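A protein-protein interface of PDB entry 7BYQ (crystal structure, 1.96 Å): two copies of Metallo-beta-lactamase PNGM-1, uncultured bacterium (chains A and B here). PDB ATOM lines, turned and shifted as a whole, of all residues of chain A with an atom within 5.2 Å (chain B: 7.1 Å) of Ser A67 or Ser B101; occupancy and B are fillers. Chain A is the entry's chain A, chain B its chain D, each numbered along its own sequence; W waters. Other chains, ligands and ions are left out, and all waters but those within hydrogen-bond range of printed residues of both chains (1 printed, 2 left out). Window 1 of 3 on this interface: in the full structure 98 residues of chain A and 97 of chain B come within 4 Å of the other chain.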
ATOM      1  N   ALA A  42      -0.415  14.475 -16.433  1.00  0.00           N
ATOM      2  CA  ALA A  42      -0.536  15.288 -15.202  1.00  0.00           C
ATOM      3  C   ALA A  42      -0.858  14.373 -14.010  1.00  0.00           C
ATOM      4  O   ALA A  42      -1.513  13.337 -14.207  1.00  0.00           O
ATOM      5  CB  ALA A  42      -1.588  16.352 -15.401  1.00  0.00           C
ATOM      6  N   ALA A  47       4.587  16.862 -10.269  1.00  0.00           N
ATOM      7  CA  ALA A  47       4.758  17.836 -11.367  1.00  0.00           C
ATOM      8  C   ALA A  47       5.711  17.260 -12.430  1.00  0.00           C
ATOM      9  O   ALA A  47       6.540  16.372 -12.083  1.00  0.00           O
ATOM     10  CB  ALA A  47       5.261  19.150 -10.817  1.00  0.00           C
ATOM     11  N   ALA A  48       5.570  17.728 -13.684  1.00  0.00           N
ATOM     12  CA  ALA A  48       6.505  17.494 -14.811  1.00  0.00           C
ATOM     13  C   ALA A  48       7.859  18.102 -14.454  1.00  0.00           C
ATOM     14  O   ALA A  48       7.860  19.165 -13.788  1.00  0.00           O
ATOM     15  CB  ALA A  48       5.971  18.121 -16.086  1.00  0.00           C
ATOM     16  N   ILE A  65      11.082  23.655 -16.268  1.00  0.00           N
ATOM     17  CA  ILE A  65       9.906  24.284 -15.599  1.00  0.00           C
ATOM     18  C   ILE A  65       8.634  23.764 -16.280  1.00  0.00           C
ATOM     19  O   ILE A  65       7.815  24.578 -16.729  1.00  0.00           O
ATOM     20  CB  ILE A  65      10.008  25.827 -15.608  1.00  0.00           C
ATOM     21  CG1 ILE A  65       8.717  26.498 -15.134  1.00  0.00           C
ATOM     22  CG2 ILE A  65      10.436  26.343 -16.974  1.00  0.00           C
ATOM     23  CD1 ILE A  65       8.907  27.882 -14.503  1.00  0.00           C
ATOM     24  N   GLY A  66       8.486  22.442 -16.330  1.00  0.00           N
ATOM     25  CA  GLY A  66       7.351  21.728 -16.939  1.00  0.00           C
ATOM     26  C   GLY A  66       6.025  21.939 -16.229  1.00  0.00           C
ATOM     27  O   GLY A  66       5.982  22.568 -15.162  1.00  0.00           O
ATOM     28  N   SER A  67       4.968  21.417 -16.839  1.00  0.00           N
ATOM     29  CA  SER A  67       3.549  21.560 -16.433  1.00  0.00           C
ATOM     30  C   SER A  67       3.401  21.190 -14.956  1.00  0.00           C
ATOM     31  O   SER A  67       3.982  20.157 -14.549  1.00  0.00           O
ATOM     32  CB  SER A  67       2.687  20.715 -17.313  1.00  0.00           C
ATOM     33  OG  SER A  67       2.944  21.012 -18.678  1.00  0.00           O
ATOM     34  N   GLY A  68       2.714  22.045 -14.199  1.00  0.00           N
ATOM     35  CA  GLY A  68       2.342  21.831 -12.789  1.00  0.00           C
ATOM     36  C   GLY A  68       3.483  22.095 -11.820  1.00  0.00           C
ATOM     37  O   GLY A  68       3.309  21.759 -10.627  1.00  0.00           O
ATOM     38  N   SER A  69       4.603  22.677 -12.269  1.00  0.00           N
ATOM     39  CA  SER A  69       5.869  22.742 -11.481  1.00  0.00           C
ATOM     40  C   SER A  69       5.916  24.003 -10.614  1.00  0.00           C
ATOM     41  O   SER A  69       6.682  24.010  -9.615  1.00  0.00           O
ATOM     42  CB  SER A  69       7.088  22.642 -12.365  1.00  0.00           C
ATOM     43  OG  SER A  69       7.408  23.894 -12.961  1.00  0.00           O
ATOM     44  N   THR A  93       6.422  20.067 -23.588  1.00  0.00           N
ATOM     45  CA  THR A  93       5.516  20.812 -22.671  1.00  0.00           C
ATOM     46  C   THR A  93       5.891  20.446 -21.234  1.00  0.00           C
ATOM     47  O   THR A  93       5.941  21.343 -20.391  1.00  0.00           O
ATOM     48  CB  THR A  93       4.035  20.505 -22.936  1.00  0.00           C
ATOM     49  OG1 THR A  93       3.810  19.106 -22.765  1.00  0.00           O
ATOM     50  CG2 THR A  93       3.571  20.909 -24.318  1.00  0.00           C
ATOM     51  N   ASP A  94       6.230  19.171 -21.027  1.00  0.00           N
ATOM     52  CA  ASP A  94       6.547  18.549 -19.717  1.00  0.00           C
ATOM     53  C   ASP A  94       7.876  19.071 -19.178  1.00  0.00           C
ATOM     54  O   ASP A  94       8.328  18.515 -18.197  1.00  0.00           O
ATOM     55  CB  ASP A  94       6.626  17.030 -19.873  1.00  0.00           C
ATOM     56  CG  ASP A  94       5.270  16.394 -20.043  1.00  0.00           C
ATOM     57  OD1 ASP A  94       4.327  16.822 -19.321  1.00  0.00           O
ATOM     58  OD2 ASP A  94       5.173  15.459 -20.868  1.00  0.00           O
ATOM     59  N   HIS A  95       8.482  20.077 -19.810  1.00  0.00           N
ATOM     60  CA  HIS A  95       9.857  20.547 -19.496  1.00  0.00           C
ATOM     61  C   HIS A  95       9.940  22.083 -19.495  1.00  0.00           C
ATOM     62  O   HIS A  95      10.933  22.580 -18.952  1.00  0.00           O
ATOM     63  CB  HIS A  95      10.877  19.877 -20.442  1.00  0.00           C
ATOM     64  CG  HIS A  95      11.285  18.505 -20.016  1.00  0.00           C
ATOM     65  ND1 HIS A  95      12.421  18.265 -19.254  1.00  0.00           N
ATOM     66  CD2 HIS A  95      10.717  17.300 -20.223  1.00  0.00           C
ATOM     67  CE1 HIS A  95      12.527  16.981 -19.002  1.00  0.00           C
ATOM     68  NE2 HIS A  95      11.502  16.364 -19.597  1.00  0.00           N
ATOM     69  N   GLY A  97       6.480  23.899 -19.956  1.00  0.00           N
ATOM     70  CA  GLY A  97       5.040  24.218 -19.913  1.00  0.00           C
ATOM     71  C   GLY A  97       4.687  25.386 -19.001  1.00  0.00           C
ATOM     72  O   GLY A  97       3.758  26.159 -19.383  1.00  0.00           O
ATOM     73  N   ASP A  98       5.338  25.511 -17.831  1.00  0.00           N
ATOM     74  CA  ASP A  98       4.947  26.503 -16.783  1.00  0.00           C
ATOM     75  C   ASP A  98       5.861  27.736 -16.835  1.00  0.00           C
ATOM     76  O   ASP A  98       5.672  28.656 -15.999  1.00  0.00           O
ATOM     77  CB  ASP A  98       4.943  25.889 -15.373  1.00  0.00           C
ATOM     78  CG  ASP A  98       3.605  25.329 -14.908  1.00  0.00           C
ATOM     79  OD1 ASP A  98       2.525  25.853 -15.308  1.00  0.00           O
ATOM     80  OD2 ASP A  98       3.647  24.391 -14.100  1.00  0.00           O
ATOM     81  N   ILE B  65      -9.175  26.620 -18.166  1.00  0.00           N
ATOM     82  CA  ILE B  65      -8.194  25.522 -17.932  1.00  0.00           C
ATOM     83  C   ILE B  65      -6.834  26.180 -17.697  1.00  0.00           C
ATOM     84  O   ILE B  65      -5.972  26.078 -18.585  1.00  0.00           O
ATOM     85  CB  ILE B  65      -8.225  24.515 -19.101  1.00  0.00           C
ATOM     86  CG1 ILE B  65      -7.298  23.324 -18.841  1.00  0.00           C
ATOM     87  CG2 ILE B  65      -7.955  25.199 -20.439  1.00  0.00           C
ATOM     88  CD1 ILE B  65      -7.515  22.155 -19.764  1.00  0.00           C
ATOM     89  N   GLY B  68      -1.758  24.552 -14.001  1.00  0.00           N
ATOM     90  CA  GLY B  68      -1.782  23.570 -12.899  1.00  0.00           C
ATOM     91  C   GLY B  68      -3.153  22.985 -12.588  1.00  0.00           C
ATOM     92  O   GLY B  68      -3.332  22.546 -11.424  1.00  0.00           O
ATOM     93  N   MET B  70      -4.542  20.525 -14.679  1.00  0.00           N
ATOM     94  CA  MET B  70      -4.512  19.273 -15.483  1.00  0.00           C
ATOM     95  C   MET B  70      -4.315  18.080 -14.542  1.00  0.00           C
ATOM     96  O   MET B  70      -4.859  17.004 -14.844  1.00  0.00           O
ATOM     97  CB  MET B  70      -3.395  19.346 -16.533  1.00  0.00           C
ATOM     98  CG  MET B  70      -3.462  18.282 -17.615  1.00  0.00           C
ATOM     99  SD  MET B  70      -4.823  18.451 -18.817  1.00  0.00           S
ATOM    100  CE  MET B  70      -5.258  16.734 -19.084  1.00  0.00           C
ATOM    101  N   ALA B  71      -3.607  18.275 -13.422  1.00  0.00           N
ATOM    102  CA  ALA B  71      -3.521  17.299 -12.310  1.00  0.00           C
ATOM    103  C   ALA B  71      -4.936  16.942 -11.854  1.00  0.00           C
ATOM    104  O   ALA B  71      -5.313  15.760 -11.971  1.00  0.00           O
ATOM    105  CB  ALA B  71      -2.692  17.853 -11.173  1.00  0.00           C
ATOM    106  N   TRP B  96      -6.164  29.716 -19.331  1.00  0.00           N
ATOM    107  CA  TRP B  96      -5.932  28.795 -20.473  1.00  0.00           C
ATOM    108  C   TRP B  96      -4.522  28.165 -20.474  1.00  0.00           C
ATOM    109  O   TRP B  96      -4.388  27.083 -21.035  1.00  0.00           O
ATOM    110  CB  TRP B  96      -6.309  29.516 -21.773  1.00  0.00           C
ATOM    111  CG  TRP B  96      -5.361  30.558 -22.286  1.00  0.00           C
ATOM    112  CD1 TRP B  96      -5.163  31.831 -21.839  1.00  0.00           C
ATOM    113  CD2 TRP B  96      -4.542  30.418 -23.455  1.00  0.00           C
ATOM    114  NE1 TRP B  96      -4.241  32.475 -22.625  1.00  0.00           N
ATOM    115  CE2 TRP B  96      -3.834  31.625 -23.617  1.00  0.00           C
ATOM    116  CE3 TRP B  96      -4.313  29.367 -24.351  1.00  0.00           C
ATOM    117  CZ2 TRP B  96      -2.930  31.814 -24.660  1.00  0.00           C
ATOM    118  CZ3 TRP B  96      -3.420  29.558 -25.379  1.00  0.00           C
ATOM    119  CH2 TRP B  96      -2.737  30.762 -25.525  1.00  0.00           C
ATOM    120  N   GLY B  97      -3.524  28.784 -19.847  1.00  0.00           N
ATOM    121  CA  GLY B  97      -2.186  28.223 -19.551  1.00  0.00           C
ATOM    122  C   GLY B  97      -2.035  26.696 -19.618  1.00  0.00           C
ATOM    123  O   GLY B  97      -0.959  26.273 -20.089  1.00  0.00           O
ATOM    124  N   ASP B  98      -2.989  25.887 -19.114  1.00  0.00           N
ATOM    125  CA  ASP B  98      -2.967  24.395 -19.226  1.00  0.00           C
ATOM    126  C   ASP B  98      -3.847  23.899 -20.381  1.00  0.00           C
ATOM    127  O   ASP B  98      -4.431  22.795 -20.269  1.00  0.00           O
ATOM    128  CB  ASP B  98      -3.422  23.688 -17.944  1.00  0.00           C
ATOM    129  CG  ASP B  98      -2.261  23.164 -17.124  1.00  0.00           C
ATOM    130  OD1 ASP B  98      -1.112  23.580 -17.422  1.00  0.00           O
ATOM    131  OD2 ASP B  98      -2.510  22.350 -16.200  1.00  0.00           O
ATOM    132  N   LEU B  99      -3.915  24.649 -21.476  1.00  0.00           N
ATOM    133  CA  LEU B  99      -4.463  24.111 -22.748  1.00  0.00           C
ATOM    134  C   LEU B  99      -3.357  23.283 -23.405  1.00  0.00           C
ATOM    135  O   LEU B  99      -3.681  22.323 -24.115  1.00  0.00           O
ATOM    136  CB  LEU B  99      -4.959  25.258 -23.637  1.00  0.00           C
ATOM    137  CG  LEU B  99      -5.431  24.839 -25.033  1.00  0.00           C
ATOM    138  CD1 LEU B  99      -6.556  23.818 -24.929  1.00  0.00           C
ATOM    139  CD2 LEU B  99      -5.895  26.053 -25.824  1.00  0.00           C
ATOM    140  N   VAL B 100      -2.099  23.591 -23.092  1.00  0.00           N
ATOM    141  CA  VAL B 100      -0.901  22.999 -23.748  1.00  0.00           C
ATOM    142  C   VAL B 100      -0.546  21.661 -23.079  1.00  0.00           C
ATOM    143  O   VAL B 100      -0.036  20.759 -23.789  1.00  0.00           O
ATOM    144  CB  VAL B 100       0.272  23.994 -23.749  1.00  0.00           C
ATOM    145  CG1 VAL B 100       0.871  24.183 -22.357  1.00  0.00           C
ATOM    146  CG2 VAL B 100       1.329  23.575 -24.755  1.00  0.00           C
ATOM    147  N   SER B 101      -0.840  21.489 -21.788  1.00  0.00           N
ATOM    148  CA  SER B 101      -0.718  20.169 -21.116  1.00  0.00           C
ATOM    149  C   SER B 101      -1.887  19.275 -21.539  1.00  0.00           C
ATOM    150  O   SER B 101      -1.670  18.066 -21.689  1.00  0.00           O
ATOM    151  CB  SER B 101      -0.626  20.293 -19.620  1.00  0.00           C
ATOM    152  OG  SER B 101      -0.505  19.004 -19.037  1.00  0.00           O
ATOM    153  N   MET B 102      -3.083  19.851 -21.721  1.00  0.00           N
ATOM    154  CA  MET B 102      -4.270  19.160 -22.299  1.00  0.00           C
ATOM    155  C   MET B 102      -3.895  18.607 -23.681  1.00  0.00           C
ATOM    156  O   MET B 102      -4.124  17.416 -23.931  1.00  0.00           O
ATOM    157  CB  MET B 102      -5.454  20.127 -22.419  1.00  0.00           C
ATOM    158  CG  MET B 102      -6.658  19.559 -23.154  1.00  0.00           C
ATOM    159  SD  MET B 102      -7.400  18.125 -22.345  1.00  0.00           S
ATOM    160  CE  MET B 102      -7.907  18.862 -20.790  1.00  0.00           C
ATOM    161  N   TRP B 103      -3.286  19.442 -24.524  1.00  0.00           N
ATOM    162  CA  TRP B 103      -2.985  19.149 -25.950  1.00  0.00           C
ATOM    163  C   TRP B 103      -1.905  18.063 -26.058  1.00  0.00           C
ATOM    164  O   TRP B 103      -2.165  17.037 -26.707  1.00  0.00           O
ATOM    165  CB  TRP B 103      -2.580  20.444 -26.659  1.00  0.00           C
ATOM    166  CG  TRP B 103      -1.963  20.258 -28.011  1.00  0.00           C
ATOM    167  CD1 TRP B 103      -2.588  19.870 -29.162  1.00  0.00           C
ATOM    168  CD2 TRP B 103      -0.588  20.486 -28.358  1.00  0.00           C
ATOM    169  NE1 TRP B 103      -1.690  19.829 -30.194  1.00  0.00           N
ATOM    170  CE2 TRP B 103      -0.462  20.223 -29.738  1.00  0.00           C
ATOM    171  CE3 TRP B 103       0.548  20.885 -27.645  1.00  0.00           C
ATOM    172  CZ2 TRP B 103       0.761  20.319 -30.400  1.00  0.00           C
ATOM    173  CZ3 TRP B 103       1.749  21.004 -28.309  1.00  0.00           C
ATOM    174  CH2 TRP B 103       1.853  20.719 -29.669  1.00  0.00           C
ATOM    175  N   ALA B 104      -0.742  18.284 -25.446  1.00  0.00           N
ATOM    176  CA  ALA B 104       0.383  17.321 -25.377  1.00  0.00           C
ATOM    177  C   ALA B 104      -0.033  16.090 -24.561  1.00  0.00           C
ATOM    178  O   ALA B 104       0.247  14.958 -25.010  1.00  0.00           O
ATOM    179  CB  ALA B 104       1.604  17.984 -24.793  1.00  0.00           C
ATOM    180  N   GLY B 105      -0.674  16.300 -23.407  1.00  0.00           N
ATOM    181  CA  GLY B 105      -1.192  15.213 -22.553  1.00  0.00           C
ATOM    182  C   GLY B 105      -2.219  14.367 -23.282  1.00  0.00           C
ATOM    183  O   GLY B 105      -1.840  13.293 -23.777  1.00  0.00           O
ATOM    184  N   GLY B 106      -3.468  14.844 -23.349  1.00  0.00           N
ATOM    185  CA  GLY B 106      -4.602  14.187 -24.032  1.00  0.00           C
ATOM    186  C   GLY B 106      -4.174  13.378 -25.247  1.00  0.00           C
ATOM    187  O   GLY B 106      -4.650  12.225 -25.393  1.00  0.00           O
ATOM    188  N   TRP B 107      -3.299  13.931 -26.090  1.00  0.00           N
ATOM    189  CA  TRP B 107      -2.709  13.209 -27.255  1.00  0.00           C
ATOM    190  C   TRP B 107      -2.139  11.861 -26.785  1.00  0.00           C
ATOM    191  O   TRP B 107      -2.564  10.822 -27.344  1.00  0.00           O
ATOM    192  CB  TRP B 107      -1.647  14.070 -27.944  1.00  0.00           C
ATOM    193  CG  TRP B 107      -1.276  13.646 -29.333  1.00  0.00           C
ATOM    194  CD1 TRP B 107      -1.355  12.396 -29.879  1.00  0.00           C
ATOM    195  CD2 TRP B 107      -0.741  14.496 -30.365  1.00  0.00           C
ATOM    196  NE1 TRP B 107      -0.921  12.410 -31.179  1.00  0.00           N
ATOM    197  CE2 TRP B 107      -0.532  13.683 -31.504  1.00  0.00           C
ATOM    198  CE3 TRP B 107      -0.425  15.860 -30.442  1.00  0.00           C
ATOM    199  CZ2 TRP B 107      -0.011  14.194 -32.691  1.00  0.00           C
ATOM    200  CZ3 TRP B 107       0.080  16.364 -31.621  1.00  0.00           C
ATOM    201  CH2 TRP B 107       0.285  15.539 -32.728  1.00  0.00           C
ATOM    202  N   ARG B 111      -6.570  10.773 -26.822  1.00  0.00           N
ATOM    203  CA  ARG B 111      -7.443  11.631 -27.671  1.00  0.00           C
ATOM    204  C   ARG B 111      -7.129  11.327 -29.141  1.00  0.00           C
ATOM    205  O   ARG B 111      -5.963  11.495 -29.537  1.00  0.00           O
ATOM    206  CB  ARG B 111      -7.259  13.123 -27.363  1.00  0.00           C
ATOM    207  CG  ARG B 111      -7.947  14.047 -28.361  1.00  0.00           C
ATOM    208  CD  ARG B 111      -7.753  15.528 -28.079  1.00  0.00           C
ATOM    209  NE  ARG B 111      -6.464  16.004 -28.567  1.00  0.00           N
ATOM    210  CZ  ARG B 111      -5.405  16.276 -27.806  1.00  0.00           C
ATOM    211  NH1 ARG B 111      -5.460  16.136 -26.493  1.00  0.00           N
ATOM    212  NH2 ARG B 111      -4.285  16.697 -28.367  1.00  0.00           N
ATOM    213  N   MET B 136       0.418  29.427 -29.973  1.00  0.00           N
ATOM    214  CA  MET B 136       0.688  28.426 -28.917  1.00  0.00           C
ATOM    215  C   MET B 136       1.225  27.181 -29.628  1.00  0.00           C
ATOM    216  O   MET B 136       2.345  26.773 -29.328  1.00  0.00           O
ATOM    217  CB  MET B 136      -0.592  28.117 -28.144  1.00  0.00           C
ATOM    218  CG  MET B 136      -0.363  27.439 -26.813  1.00  0.00           C
ATOM    219  SD  MET B 136      -1.812  26.468 -26.413  1.00  0.00           S
ATOM    220  CE  MET B 136      -1.606  25.114 -27.566  1.00  0.00           C
ATOM    221  N   TYR B 140       5.225  25.319 -29.344  1.00  0.00           N
ATOM    222  CA  TYR B 140       5.545  23.891 -29.100  1.00  0.00           C
ATOM    223  C   TYR B 140       5.679  23.171 -30.454  1.00  0.00           C
ATOM    224  O   TYR B 140       5.469  21.950 -30.511  1.00  0.00           O
ATOM    225  CB  TYR B 140       4.510  23.328 -28.124  1.00  0.00           C
ATOM    226  CG  TYR B 140       4.546  24.008 -26.777  1.00  0.00           C
ATOM    227  CD1 TYR B 140       5.284  23.479 -25.733  1.00  0.00           C
ATOM    228  CD2 TYR B 140       3.869  25.198 -26.545  1.00  0.00           C
ATOM    229  CE1 TYR B 140       5.351  24.109 -24.504  1.00  0.00           C
ATOM    230  CE2 TYR B 140       3.929  25.843 -25.318  1.00  0.00           C
ATOM    231  CZ  TYR B 140       4.672  25.294 -24.288  1.00  0.00           C
ATOM    232  OH  TYR B 140       4.754  25.911 -23.071  1.00  0.00           O
ATOM    233  N   ARG B 147       6.662  14.686 -32.321  1.00  0.00           N
ATOM    234  CA  ARG B 147       5.542  13.824 -31.854  1.00  0.00           C
ATOM    235  C   ARG B 147       4.877  13.133 -33.053  1.00  0.00           C
ATOM    236  O   ARG B 147       4.749  11.901 -33.017  1.00  0.00           O
ATOM    237  CB  ARG B 147       4.539  14.676 -31.073  1.00  0.00           C
ATOM    238  CG  ARG B 147       3.255  13.957 -30.692  1.00  0.00           C
ATOM    239  CD  ARG B 147       2.547  14.656 -29.545  1.00  0.00           C
ATOM    240  NE  ARG B 147       3.317  14.517 -28.315  1.00  0.00           N
ATOM    241  CZ  ARG B 147       2.811  14.513 -27.082  1.00  0.00           C
ATOM    242  NH1 ARG B 147       1.509  14.638 -26.897  1.00  0.00           N
ATOM    243  NH2 ARG B 147       3.612  14.373 -26.039  1.00  0.00           N
HETATM  244  O   HOH W   1       0.552  27.304 -17.707  1.00  0.00           O
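N of Met B70 lies within hydrogen-bond range of OD2 of Asp B98 (3.1 Å).
O of Ser A67 lies within hydrogen-bond range of N of Ala A48 (3.0 Å).
The backbone NH of Met B102 lies close to the side-chain sulfur of Met B70.
OG of Ser A67 sits at hydrogen-bond distance from O of Thr A93, at 3.5 Å.
Among the printed residues, merely in contact across the chains: Ala A42 with Met B70 (3.3 Å), Ala A42 with Ala B71 (3.4 Å), Ser A67 with Ser B101 (3.8 Å), Thr A93 with Val B100 (3.5 Å), Thr A93 with Ala B104 (3.2 Å), Thr A93 with Tyr B140 (3.4 Å) and Gly A97 with Tyr B140 (3.6 Å).
Printed residues of chain B within 4 Å of Ala A42: Met B70 and Ala B71.
Of chain B, only Ser B101 (3.8 Å) comes within 4 Å of Ser A67.
Of the printed residues of chain B, Thr A93 touches Val B100, Ala B104 and Tyr B140.
Met B102 touches none of the printed residues of chain A.
Of the printed residues of chain A, Tyr B140 touches Thr A93 (3.4 Å) and Gly A97 (3.6 Å).
The nearest residue of chain A that does not touch Ser B101 is Ala A42 (4.6 Å).
Of the 20 printed residues of chain B, 6 touch a printed residue of chain A.
Hydrophobic or aromatic side chains of chain B that line the printed part of chain A: Met B70, Val B100, Ala B104 and Tyr B140.
Of the 13 printed residues of chain A, 4 touch a printed residue of chain B.
Hydrophobic or aromatic side chains of chain A that line the printed part of chain B: Ala A42.
Among the printed residues, 7 pairs touch across the chains.
4 positions are printed for both chains.
Water W1 bridges O of Gly B97 (3.0 Å) and OD1 of Asp A98 (3.4 Å).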
